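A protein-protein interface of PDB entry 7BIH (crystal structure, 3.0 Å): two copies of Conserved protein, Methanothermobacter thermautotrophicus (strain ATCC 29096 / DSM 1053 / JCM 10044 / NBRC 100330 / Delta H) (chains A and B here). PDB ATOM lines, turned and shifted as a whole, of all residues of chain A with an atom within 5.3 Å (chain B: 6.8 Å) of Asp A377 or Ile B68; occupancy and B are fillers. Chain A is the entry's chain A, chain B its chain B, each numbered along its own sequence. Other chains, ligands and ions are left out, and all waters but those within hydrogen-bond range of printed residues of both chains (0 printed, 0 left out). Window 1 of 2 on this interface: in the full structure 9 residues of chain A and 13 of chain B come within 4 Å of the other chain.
The side-chain carboxylate (OD2) of Asp A377 sits at hydrogen-bond distance from the side-chain hydroxyl (OG) of Ser B69, 2.9 Å away. The guanidinium group (NH2) of Arg B39 lies within salt-bridge range of the side-chain carboxylate (OD2) of Asp A379 (2.9 Å). The side-chain carboxylate (OD2) of Asp A379 lies within hydrogen-bond range of a ring nitrogen (NE2) of His B67, 3.4 Å away.
O of Ile B38 sits at hydrogen-bond distance from N of His B67 (2.8 Å). A ring nitrogen (ND1) of His B67 sits at hydrogen-bond distance from the guanidinium group (NH1) of Arg B39 (2.9 Å). NH2 of Arg B39 is in hydrogen-bond range of OG of Ser B69 (2.7 Å). N of Ile B40 lies within hydrogen-bond range of O of His B67 (2.8 Å). O of Ile B40 is in hydrogen-bond range of N of Ser B69. The backbone NH of Ser B42 is in hydrogen-bond range of the backbone carbonyl oxygen of Ser B69, 3.0 Å away.
Among the printed residues, merely in contact across the chains: Lys A374 with His B67 (3.96 Å), Asp A377 with His B67 (3.0 Å), Asp A377 with Ile B68 (3.6 Å) and Pro A378 with His B67 (3.6 Å).
Leu A371 touches none of the printed residues of chain B. Printed residues of chain B within 4 Å of Asp A377: His B67 (3.0 Å), Ile B68 (3.6 Å) and Ser B69 (2.9 Å). Ile A380 touches none of the printed residues of chain B. Printed residues of chain A within 4 Å of Arg B39: Asp A379 (2.9 Å). Of chain A, only Asp A377 comes within 4 Å of Ile B68. Of the printed residues of chain A, Ser B69 touches Asp A377 (2.9 Å).
Of the 15 printed residues of chain B, 4 touch a printed residue of chain A. Printed residues of chain B that touch a printed residue of chain A: Arg B39, His B67, Ile B68 and Ser B69. Hydrophobic or aromatic side chains of chain B within 4 Å of the printed part of chain A: His B67. Printed residues of chain A that touch a printed residue of chain B: Lys A374, Asp A377, Pro A378 and Asp A379. Among the printed residues, Asp or Glu carboxylates within 4 Å of a Lys or Arg side-chain nitrogen of the other chain: Asp A379 with Arg B39.
No position is printed for both chains.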
ATOM      1  N   GLN A 350       7.616  -3.718  -9.606  1.00  0.00           N
ATOM      2  CA  GLN A 350       7.078  -2.551 -10.290  1.00  0.00           C
ATOM      3  C   GLN A 350       5.984  -3.024 -11.250  1.00  0.00           C
ATOM      4  O   GLN A 350       5.970  -4.176 -11.644  1.00  0.00           O
ATOM      5  CB  GLN A 350       8.176  -1.824 -11.057  1.00  0.00           C
ATOM      6  CG  GLN A 350       8.997  -2.700 -11.990  1.00  0.00           C
ATOM      7  CD  GLN A 350      10.105  -1.919 -12.629  1.00  0.00           C
ATOM      8  OE1 GLN A 350       9.894  -0.778 -13.050  1.00  0.00           O
ATOM      9  NE2 GLN A 350      11.297  -2.509 -12.695  1.00  0.00           N
ATOM     10  N   LEU A 371      13.533  -3.722 -19.588  1.00  0.00           N
ATOM     11  CA  LEU A 371      14.446  -4.020 -18.517  1.00  0.00           C
ATOM     12  C   LEU A 371      15.875  -4.121 -19.026  1.00  0.00           C
ATOM     13  O   LEU A 371      16.805  -3.639 -18.357  1.00  0.00           O
ATOM     14  CB  LEU A 371      14.052  -5.343 -17.857  1.00  0.00           C
ATOM     15  CG  LEU A 371      12.724  -5.388 -17.124  1.00  0.00           C
ATOM     16  CD1 LEU A 371      12.468  -6.832 -16.760  1.00  0.00           C
ATOM     17  CD2 LEU A 371      12.727  -4.533 -15.862  1.00  0.00           C
ATOM     18  N   LYS A 374      17.005  -0.778 -19.617  1.00  0.00           N
ATOM     19  CA  LYS A 374      17.042  -0.039 -18.363  1.00  0.00           C
ATOM     20  C   LYS A 374      16.207   1.260 -18.395  1.00  0.00           C
ATOM     21  O   LYS A 374      16.455   2.182 -17.613  1.00  0.00           O
ATOM     22  CB  LYS A 374      18.489   0.216 -17.899  1.00  0.00           C
ATOM     23  CG  LYS A 374      19.385  -1.000 -18.035  1.00  0.00           C
ATOM     24  CD  LYS A 374      20.580  -0.932 -17.089  1.00  0.00           C
ATOM     25  CE  LYS A 374      21.603  -2.030 -17.309  1.00  0.00           C
ATOM     26  NZ  LYS A 374      22.668  -2.053 -16.260  1.00  0.00           N
ATOM     27  N   ILE A 375      15.203   1.317 -19.273  1.00  0.00           N
ATOM     28  CA  ILE A 375      14.106   2.279 -19.136  1.00  0.00           C
ATOM     29  C   ILE A 375      13.541   2.133 -17.716  1.00  0.00           C
ATOM     30  O   ILE A 375      13.181   3.120 -17.042  1.00  0.00           O
ATOM     31  CB  ILE A 375      12.938   2.003 -20.124  1.00  0.00           C
ATOM     32  CG1 ILE A 375      13.340   2.295 -21.559  1.00  0.00           C
ATOM     33  CG2 ILE A 375      11.704   2.865 -19.810  1.00  0.00           C
ATOM     34  CD1 ILE A 375      12.325   1.817 -22.603  1.00  0.00           C
ATOM     35  N   LEU A 376      13.439   0.876 -17.292  1.00  0.00           N
ATOM     36  CA  LEU A 376      12.971   0.523 -15.988  1.00  0.00           C
ATOM     37  C   LEU A 376      14.073  -0.212 -15.247  1.00  0.00           C
ATOM     38  O   LEU A 376      14.915  -0.852 -15.868  1.00  0.00           O
ATOM     39  CB  LEU A 376      11.721  -0.336 -16.140  1.00  0.00           C
ATOM     40  CG  LEU A 376      10.553   0.347 -16.867  1.00  0.00           C
ATOM     41  CD1 LEU A 376       9.367  -0.593 -17.028  1.00  0.00           C
ATOM     42  CD2 LEU A 376      10.066   1.614 -16.159  1.00  0.00           C
ATOM     43  N   ASP A 377      14.040  -0.144 -13.914  1.00  0.00           N
ATOM     44  CA  ASP A 377      15.076  -0.748 -13.071  1.00  0.00           C
ATOM     45  C   ASP A 377      15.087  -2.277 -13.253  1.00  0.00           C
ATOM     46  O   ASP A 377      14.156  -2.964 -12.826  1.00  0.00           O
ATOM     47  CB  ASP A 377      14.829  -0.383 -11.612  1.00  0.00           C
ATOM     48  CG  ASP A 377      15.945  -0.831 -10.672  1.00  0.00           C
ATOM     49  OD1 ASP A 377      16.822  -1.631 -11.069  1.00  0.00           O
ATOM     50  OD2 ASP A 377      15.921  -0.393  -9.504  1.00  0.00           O
ATOM     51  N   PRO A 378      16.159  -2.817 -13.863  1.00  0.00           N
ATOM     52  CA  PRO A 378      16.194  -4.239 -14.131  1.00  0.00           C
ATOM     53  C   PRO A 378      16.272  -5.135 -12.889  1.00  0.00           C
ATOM     54  O   PRO A 378      15.946  -6.324 -12.983  1.00  0.00           O
ATOM     55  CB  PRO A 378      17.460  -4.394 -14.981  1.00  0.00           C
ATOM     56  CG  PRO A 378      18.337  -3.277 -14.570  1.00  0.00           C
ATOM     57  CD  PRO A 378      17.404  -2.153 -14.298  1.00  0.00           C
ATOM     58  N   ASP A 379      16.689  -4.579 -11.744  1.00  0.00           N
ATOM     59  CA  ASP A 379      16.725  -5.344 -10.495  1.00  0.00           C
ATOM     60  C   ASP A 379      15.347  -5.684  -9.967  1.00  0.00           C
ATOM     61  O   ASP A 379      15.219  -6.577  -9.152  1.00  0.00           O
ATOM     62  CB  ASP A 379      17.519  -4.622  -9.385  1.00  0.00           C
ATOM     63  CG  ASP A 379      19.037  -4.559  -9.670  1.00  0.00           C
ATOM     64  OD1 ASP A 379      19.587  -5.433 -10.398  1.00  0.00           O
ATOM     65  OD2 ASP A 379      19.694  -3.662  -9.113  1.00  0.00           O
ATOM     66  N   ILE A 380      14.321  -4.969 -10.415  1.00  0.00           N
ATOM     67  CA  ILE A 380      12.973  -5.102  -9.867  1.00  0.00           C
ATOM     68  C   ILE A 380      12.020  -5.819 -10.852  1.00  0.00           C
ATOM     69  O   ILE A 380      11.814  -5.340 -11.958  1.00  0.00           O
ATOM     70  CB  ILE A 380      12.431  -3.696  -9.526  1.00  0.00           C
ATOM     71  CG1 ILE A 380      13.381  -2.968  -8.585  1.00  0.00           C
ATOM     72  CG2 ILE A 380      11.076  -3.792  -8.893  1.00  0.00           C
ATOM     73  CD1 ILE A 380      12.916  -1.583  -8.189  1.00  0.00           C
ATOM     74  N   ILE B  38      28.076   3.018 -13.315  1.00  0.00           N
ATOM     75  CA  ILE B  38      27.982   3.565 -11.959  1.00  0.00           C
ATOM     76  C   ILE B  38      26.614   3.296 -11.295  1.00  0.00           C
ATOM     77  O   ILE B  38      25.559   3.564 -11.873  1.00  0.00           O
ATOM     78  CB  ILE B  38      28.321   5.061 -11.983  1.00  0.00           C
ATOM     79  CG1 ILE B  38      29.763   5.224 -12.449  1.00  0.00           C
ATOM     80  CG2 ILE B  38      28.183   5.662 -10.596  1.00  0.00           C
ATOM     81  CD1 ILE B  38      29.961   6.329 -13.438  1.00  0.00           C
ATOM     82  N   ARG B  39      26.649   2.781 -10.075  1.00  0.00           N
ATOM     83  CA  ARG B  39      25.442   2.398  -9.356  1.00  0.00           C
ATOM     84  C   ARG B  39      25.001   3.553  -8.439  1.00  0.00           C
ATOM     85  O   ARG B  39      25.716   3.917  -7.480  1.00  0.00           O
ATOM     86  CB  ARG B  39      25.713   1.126  -8.556  1.00  0.00           C
ATOM     87  CG  ARG B  39      24.487   0.454  -7.991  1.00  0.00           C
ATOM     88  CD  ARG B  39      23.695  -0.291  -9.067  1.00  0.00           C
ATOM     89  NE  ARG B  39      22.557  -0.974  -8.442  1.00  0.00           N
ATOM     90  CZ  ARG B  39      21.299  -0.520  -8.349  1.00  0.00           C
ATOM     91  NH1 ARG B  39      20.900   0.635  -8.902  1.00  0.00           N
ATOM     92  NH2 ARG B  39      20.398  -1.247  -7.695  1.00  0.00           N
ATOM     93  N   ILE B  40      23.833   4.127  -8.747  1.00  0.00           N
ATOM     94  CA  ILE B  40      23.284   5.236  -7.974  1.00  0.00           C
ATOM     95  C   ILE B  40      22.080   4.792  -7.134  1.00  0.00           C
ATOM     96  O   ILE B  40      21.115   4.251  -7.673  1.00  0.00           O
ATOM     97  CB  ILE B  40      22.860   6.390  -8.885  1.00  0.00           C
ATOM     98  CG1 ILE B  40      24.081   6.942  -9.623  1.00  0.00           C
ATOM     99  CG2 ILE B  40      22.215   7.517  -8.063  1.00  0.00           C
ATOM    100  CD1 ILE B  40      23.734   7.860 -10.784  1.00  0.00           C
ATOM    101  N   ILE B  41      22.147   5.049  -5.820  1.00  0.00           N
ATOM    102  CA  ILE B  41      21.048   4.733  -4.900  1.00  0.00           C
ATOM    103  C   ILE B  41      20.570   6.004  -4.212  1.00  0.00           C
ATOM    104  O   ILE B  41      21.361   6.695  -3.578  1.00  0.00           O
ATOM    105  CB  ILE B  41      21.445   3.732  -3.799  1.00  0.00           C
ATOM    106  CG1 ILE B  41      22.421   2.650  -4.314  1.00  0.00           C
ATOM    107  CG2 ILE B  41      20.194   3.100  -3.209  1.00  0.00           C
ATOM    108  CD1 ILE B  41      21.866   1.704  -5.369  1.00  0.00           C
ATOM    109  N   SER B  42      19.278   6.310  -4.332  1.00  0.00           N
ATOM    110  CA  SER B  42      18.738   7.531  -3.731  1.00  0.00           C
ATOM    111  C   SER B  42      17.329   7.398  -3.157  1.00  0.00           C
ATOM    112  O   SER B  42      16.672   6.373  -3.278  1.00  0.00           O
ATOM    113  CB  SER B  42      18.784   8.683  -4.754  1.00  0.00           C
ATOM    114  OG  SER B  42      18.590   9.938  -4.111  1.00  0.00           O
ATOM    115  N   ALA B  52      19.722  12.380  -7.320  1.00  0.00           N
ATOM    116  CA  ALA B  52      19.979  11.319  -8.297  1.00  0.00           C
ATOM    117  C   ALA B  52      20.118  11.869  -9.686  1.00  0.00           C
ATOM    118  O   ALA B  52      20.964  11.392 -10.470  1.00  0.00           O
ATOM    119  CB  ALA B  52      18.878  10.291  -8.278  1.00  0.00           C
ATOM    120  N   GLY B  53      19.275  12.865  -9.999  1.00  0.00           N
ATOM    121  CA  GLY B  53      19.342  13.567 -11.288  1.00  0.00           C
ATOM    122  C   GLY B  53      20.656  14.308 -11.543  1.00  0.00           C
ATOM    123  O   GLY B  53      21.194  14.280 -12.653  1.00  0.00           O
ATOM    124  N   ALA B  56      23.327  11.577 -12.292  1.00  0.00           N
ATOM    125  CA  ALA B  56      23.111  10.953 -13.602  1.00  0.00           C
ATOM    126  C   ALA B  56      23.356  11.923 -14.766  1.00  0.00           C
ATOM    127  O   ALA B  56      23.843  11.511 -15.830  1.00  0.00           O
ATOM    128  CB  ALA B  56      21.718  10.334 -13.687  1.00  0.00           C
ATOM    129  N   PHE B  66      24.841   4.728 -16.203  1.00  0.00           N
ATOM    130  CA  PHE B  66      24.464   4.645 -14.772  1.00  0.00           C
ATOM    131  C   PHE B  66      23.281   3.690 -14.559  1.00  0.00           C
ATOM    132  O   PHE B  66      22.457   3.518 -15.459  1.00  0.00           O
ATOM    133  CB  PHE B  66      24.071   6.031 -14.227  1.00  0.00           C
ATOM    134  CG  PHE B  66      23.021   6.723 -15.053  1.00  0.00           C
ATOM    135  CD1 PHE B  66      21.672   6.452 -14.885  1.00  0.00           C
ATOM    136  CD2 PHE B  66      23.384   7.618 -16.021  1.00  0.00           C
ATOM    137  CE1 PHE B  66      20.707   7.057 -15.680  1.00  0.00           C
ATOM    138  CE2 PHE B  66      22.421   8.252 -16.807  1.00  0.00           C
ATOM    139  CZ  PHE B  66      21.082   7.963 -16.641  1.00  0.00           C
ATOM    140  N   HIS B  67      23.191   3.111 -13.363  1.00  0.00           N
ATOM    141  CA  HIS B  67      22.044   2.294 -12.935  1.00  0.00           C
ATOM    142  C   HIS B  67      21.489   2.891 -11.627  1.00  0.00           C
ATOM    143  O   HIS B  67      22.175   2.897 -10.605  1.00  0.00           O
ATOM    144  CB  HIS B  67      22.524   0.858 -12.762  1.00  0.00           C
ATOM    145  CG  HIS B  67      21.486  -0.140 -12.389  1.00  0.00           C
ATOM    146  ND1 HIS B  67      20.334   0.151 -11.700  1.00  0.00           N
ATOM    147  CD2 HIS B  67      21.518  -1.480 -12.512  1.00  0.00           C
ATOM    148  CE1 HIS B  67      19.673  -0.969 -11.469  1.00  0.00           C
ATOM    149  NE2 HIS B  67      20.378  -1.974 -11.943  1.00  0.00           N
ATOM    150  N   ILE B  68      20.251   3.391 -11.677  1.00  0.00           N
ATOM    151  CA  ILE B  68      19.614   4.054 -10.553  1.00  0.00           C
ATOM    152  C   ILE B  68      18.591   3.153  -9.892  1.00  0.00           C
ATOM    153  O   ILE B  68      17.731   2.591 -10.562  1.00  0.00           O
ATOM    154  CB  ILE B  68      18.856   5.304 -11.015  1.00  0.00           C
ATOM    155  CG1 ILE B  68      19.821   6.322 -11.608  1.00  0.00           C
ATOM    156  CG2 ILE B  68      18.075   5.931  -9.851  1.00  0.00           C
ATOM    157  CD1 ILE B  68      19.147   7.403 -12.434  1.00  0.00           C
ATOM    158  N   SER B  69      18.643   3.074  -8.566  1.00  0.00           N
ATOM    159  CA  SER B  69      17.526   2.604  -7.751  1.00  0.00           C
ATOM    160  C   SER B  69      17.083   3.674  -6.757  1.00  0.00           C
ATOM    161  O   SER B  69      17.910   4.247  -6.024  1.00  0.00           O
ATOM    162  CB  SER B  69      17.918   1.349  -6.992  1.00  0.00           C
ATOM    163  OG  SER B  69      18.200   0.303  -7.911  1.00  0.00           O
ATOM    164  N   ILE B  70      15.762   3.903  -6.722  1.00  0.00           N
ATOM    165  CA  ILE B  70      15.100   4.771  -5.756  1.00  0.00           C
ATOM    166  C   ILE B  70      14.472   3.927  -4.641  1.00  0.00           C
ATOM    167  O   ILE B  70      13.753   2.945  -4.907  1.00  0.00           O
ATOM    168  CB  ILE B  70      14.022   5.618  -6.442  1.00  0.00           C
ATOM    169  CG1 ILE B  70      14.647   6.481  -7.532  1.00  0.00           C
ATOM    170  CG2 ILE B  70      13.280   6.507  -5.429  1.00  0.00           C
ATOM    171  CD1 ILE B  70      15.762   7.428  -7.067  1.00  0.00           C
ATOM    172  N   ILE B 306      12.783  11.125 -12.498  1.00  0.00           N
ATOM    173  CA  ILE B 306      14.172  11.141 -12.970  1.00  0.00           C
ATOM    174  C   ILE B 306      14.297  11.520 -14.452  1.00  0.00           C
ATOM    175  O   ILE B 306      15.242  12.214 -14.833  1.00  0.00           O
ATOM    176  CB  ILE B 306      14.868   9.799 -12.690  1.00  0.00           C
ATOM    177  CG1 ILE B 306      15.013   9.648 -11.198  1.00  0.00           C
ATOM    178  CG2 ILE B 306      16.261   9.743 -13.313  1.00  0.00           C
ATOM    179  CD1 ILE B 306      15.424   8.259 -10.823  1.00  0.00           C
ATOM    180  N   LEU B 310      16.566  14.510 -16.065  1.00  0.00           N
ATOM    181  CA  LEU B 310      17.501  14.351 -17.202  1.00  0.00           C
ATOM    182  C   LEU B 310      17.103  15.127 -18.468  1.00  0.00           C
ATOM    183  O   LEU B 310      17.894  15.196 -19.394  1.00  0.00           O
ATOM    184  CB  LEU B 310      17.675  12.866 -17.574  1.00  0.00           C
ATOM    185  CG  LEU B 310      18.432  12.007 -16.545  1.00  0.00           C
ATOM    186  CD1 LEU B 310      18.224  10.536 -16.863  1.00  0.00           C
ATOM    187  CD2 LEU B 310      19.924  12.341 -16.473  1.00  0.00           C
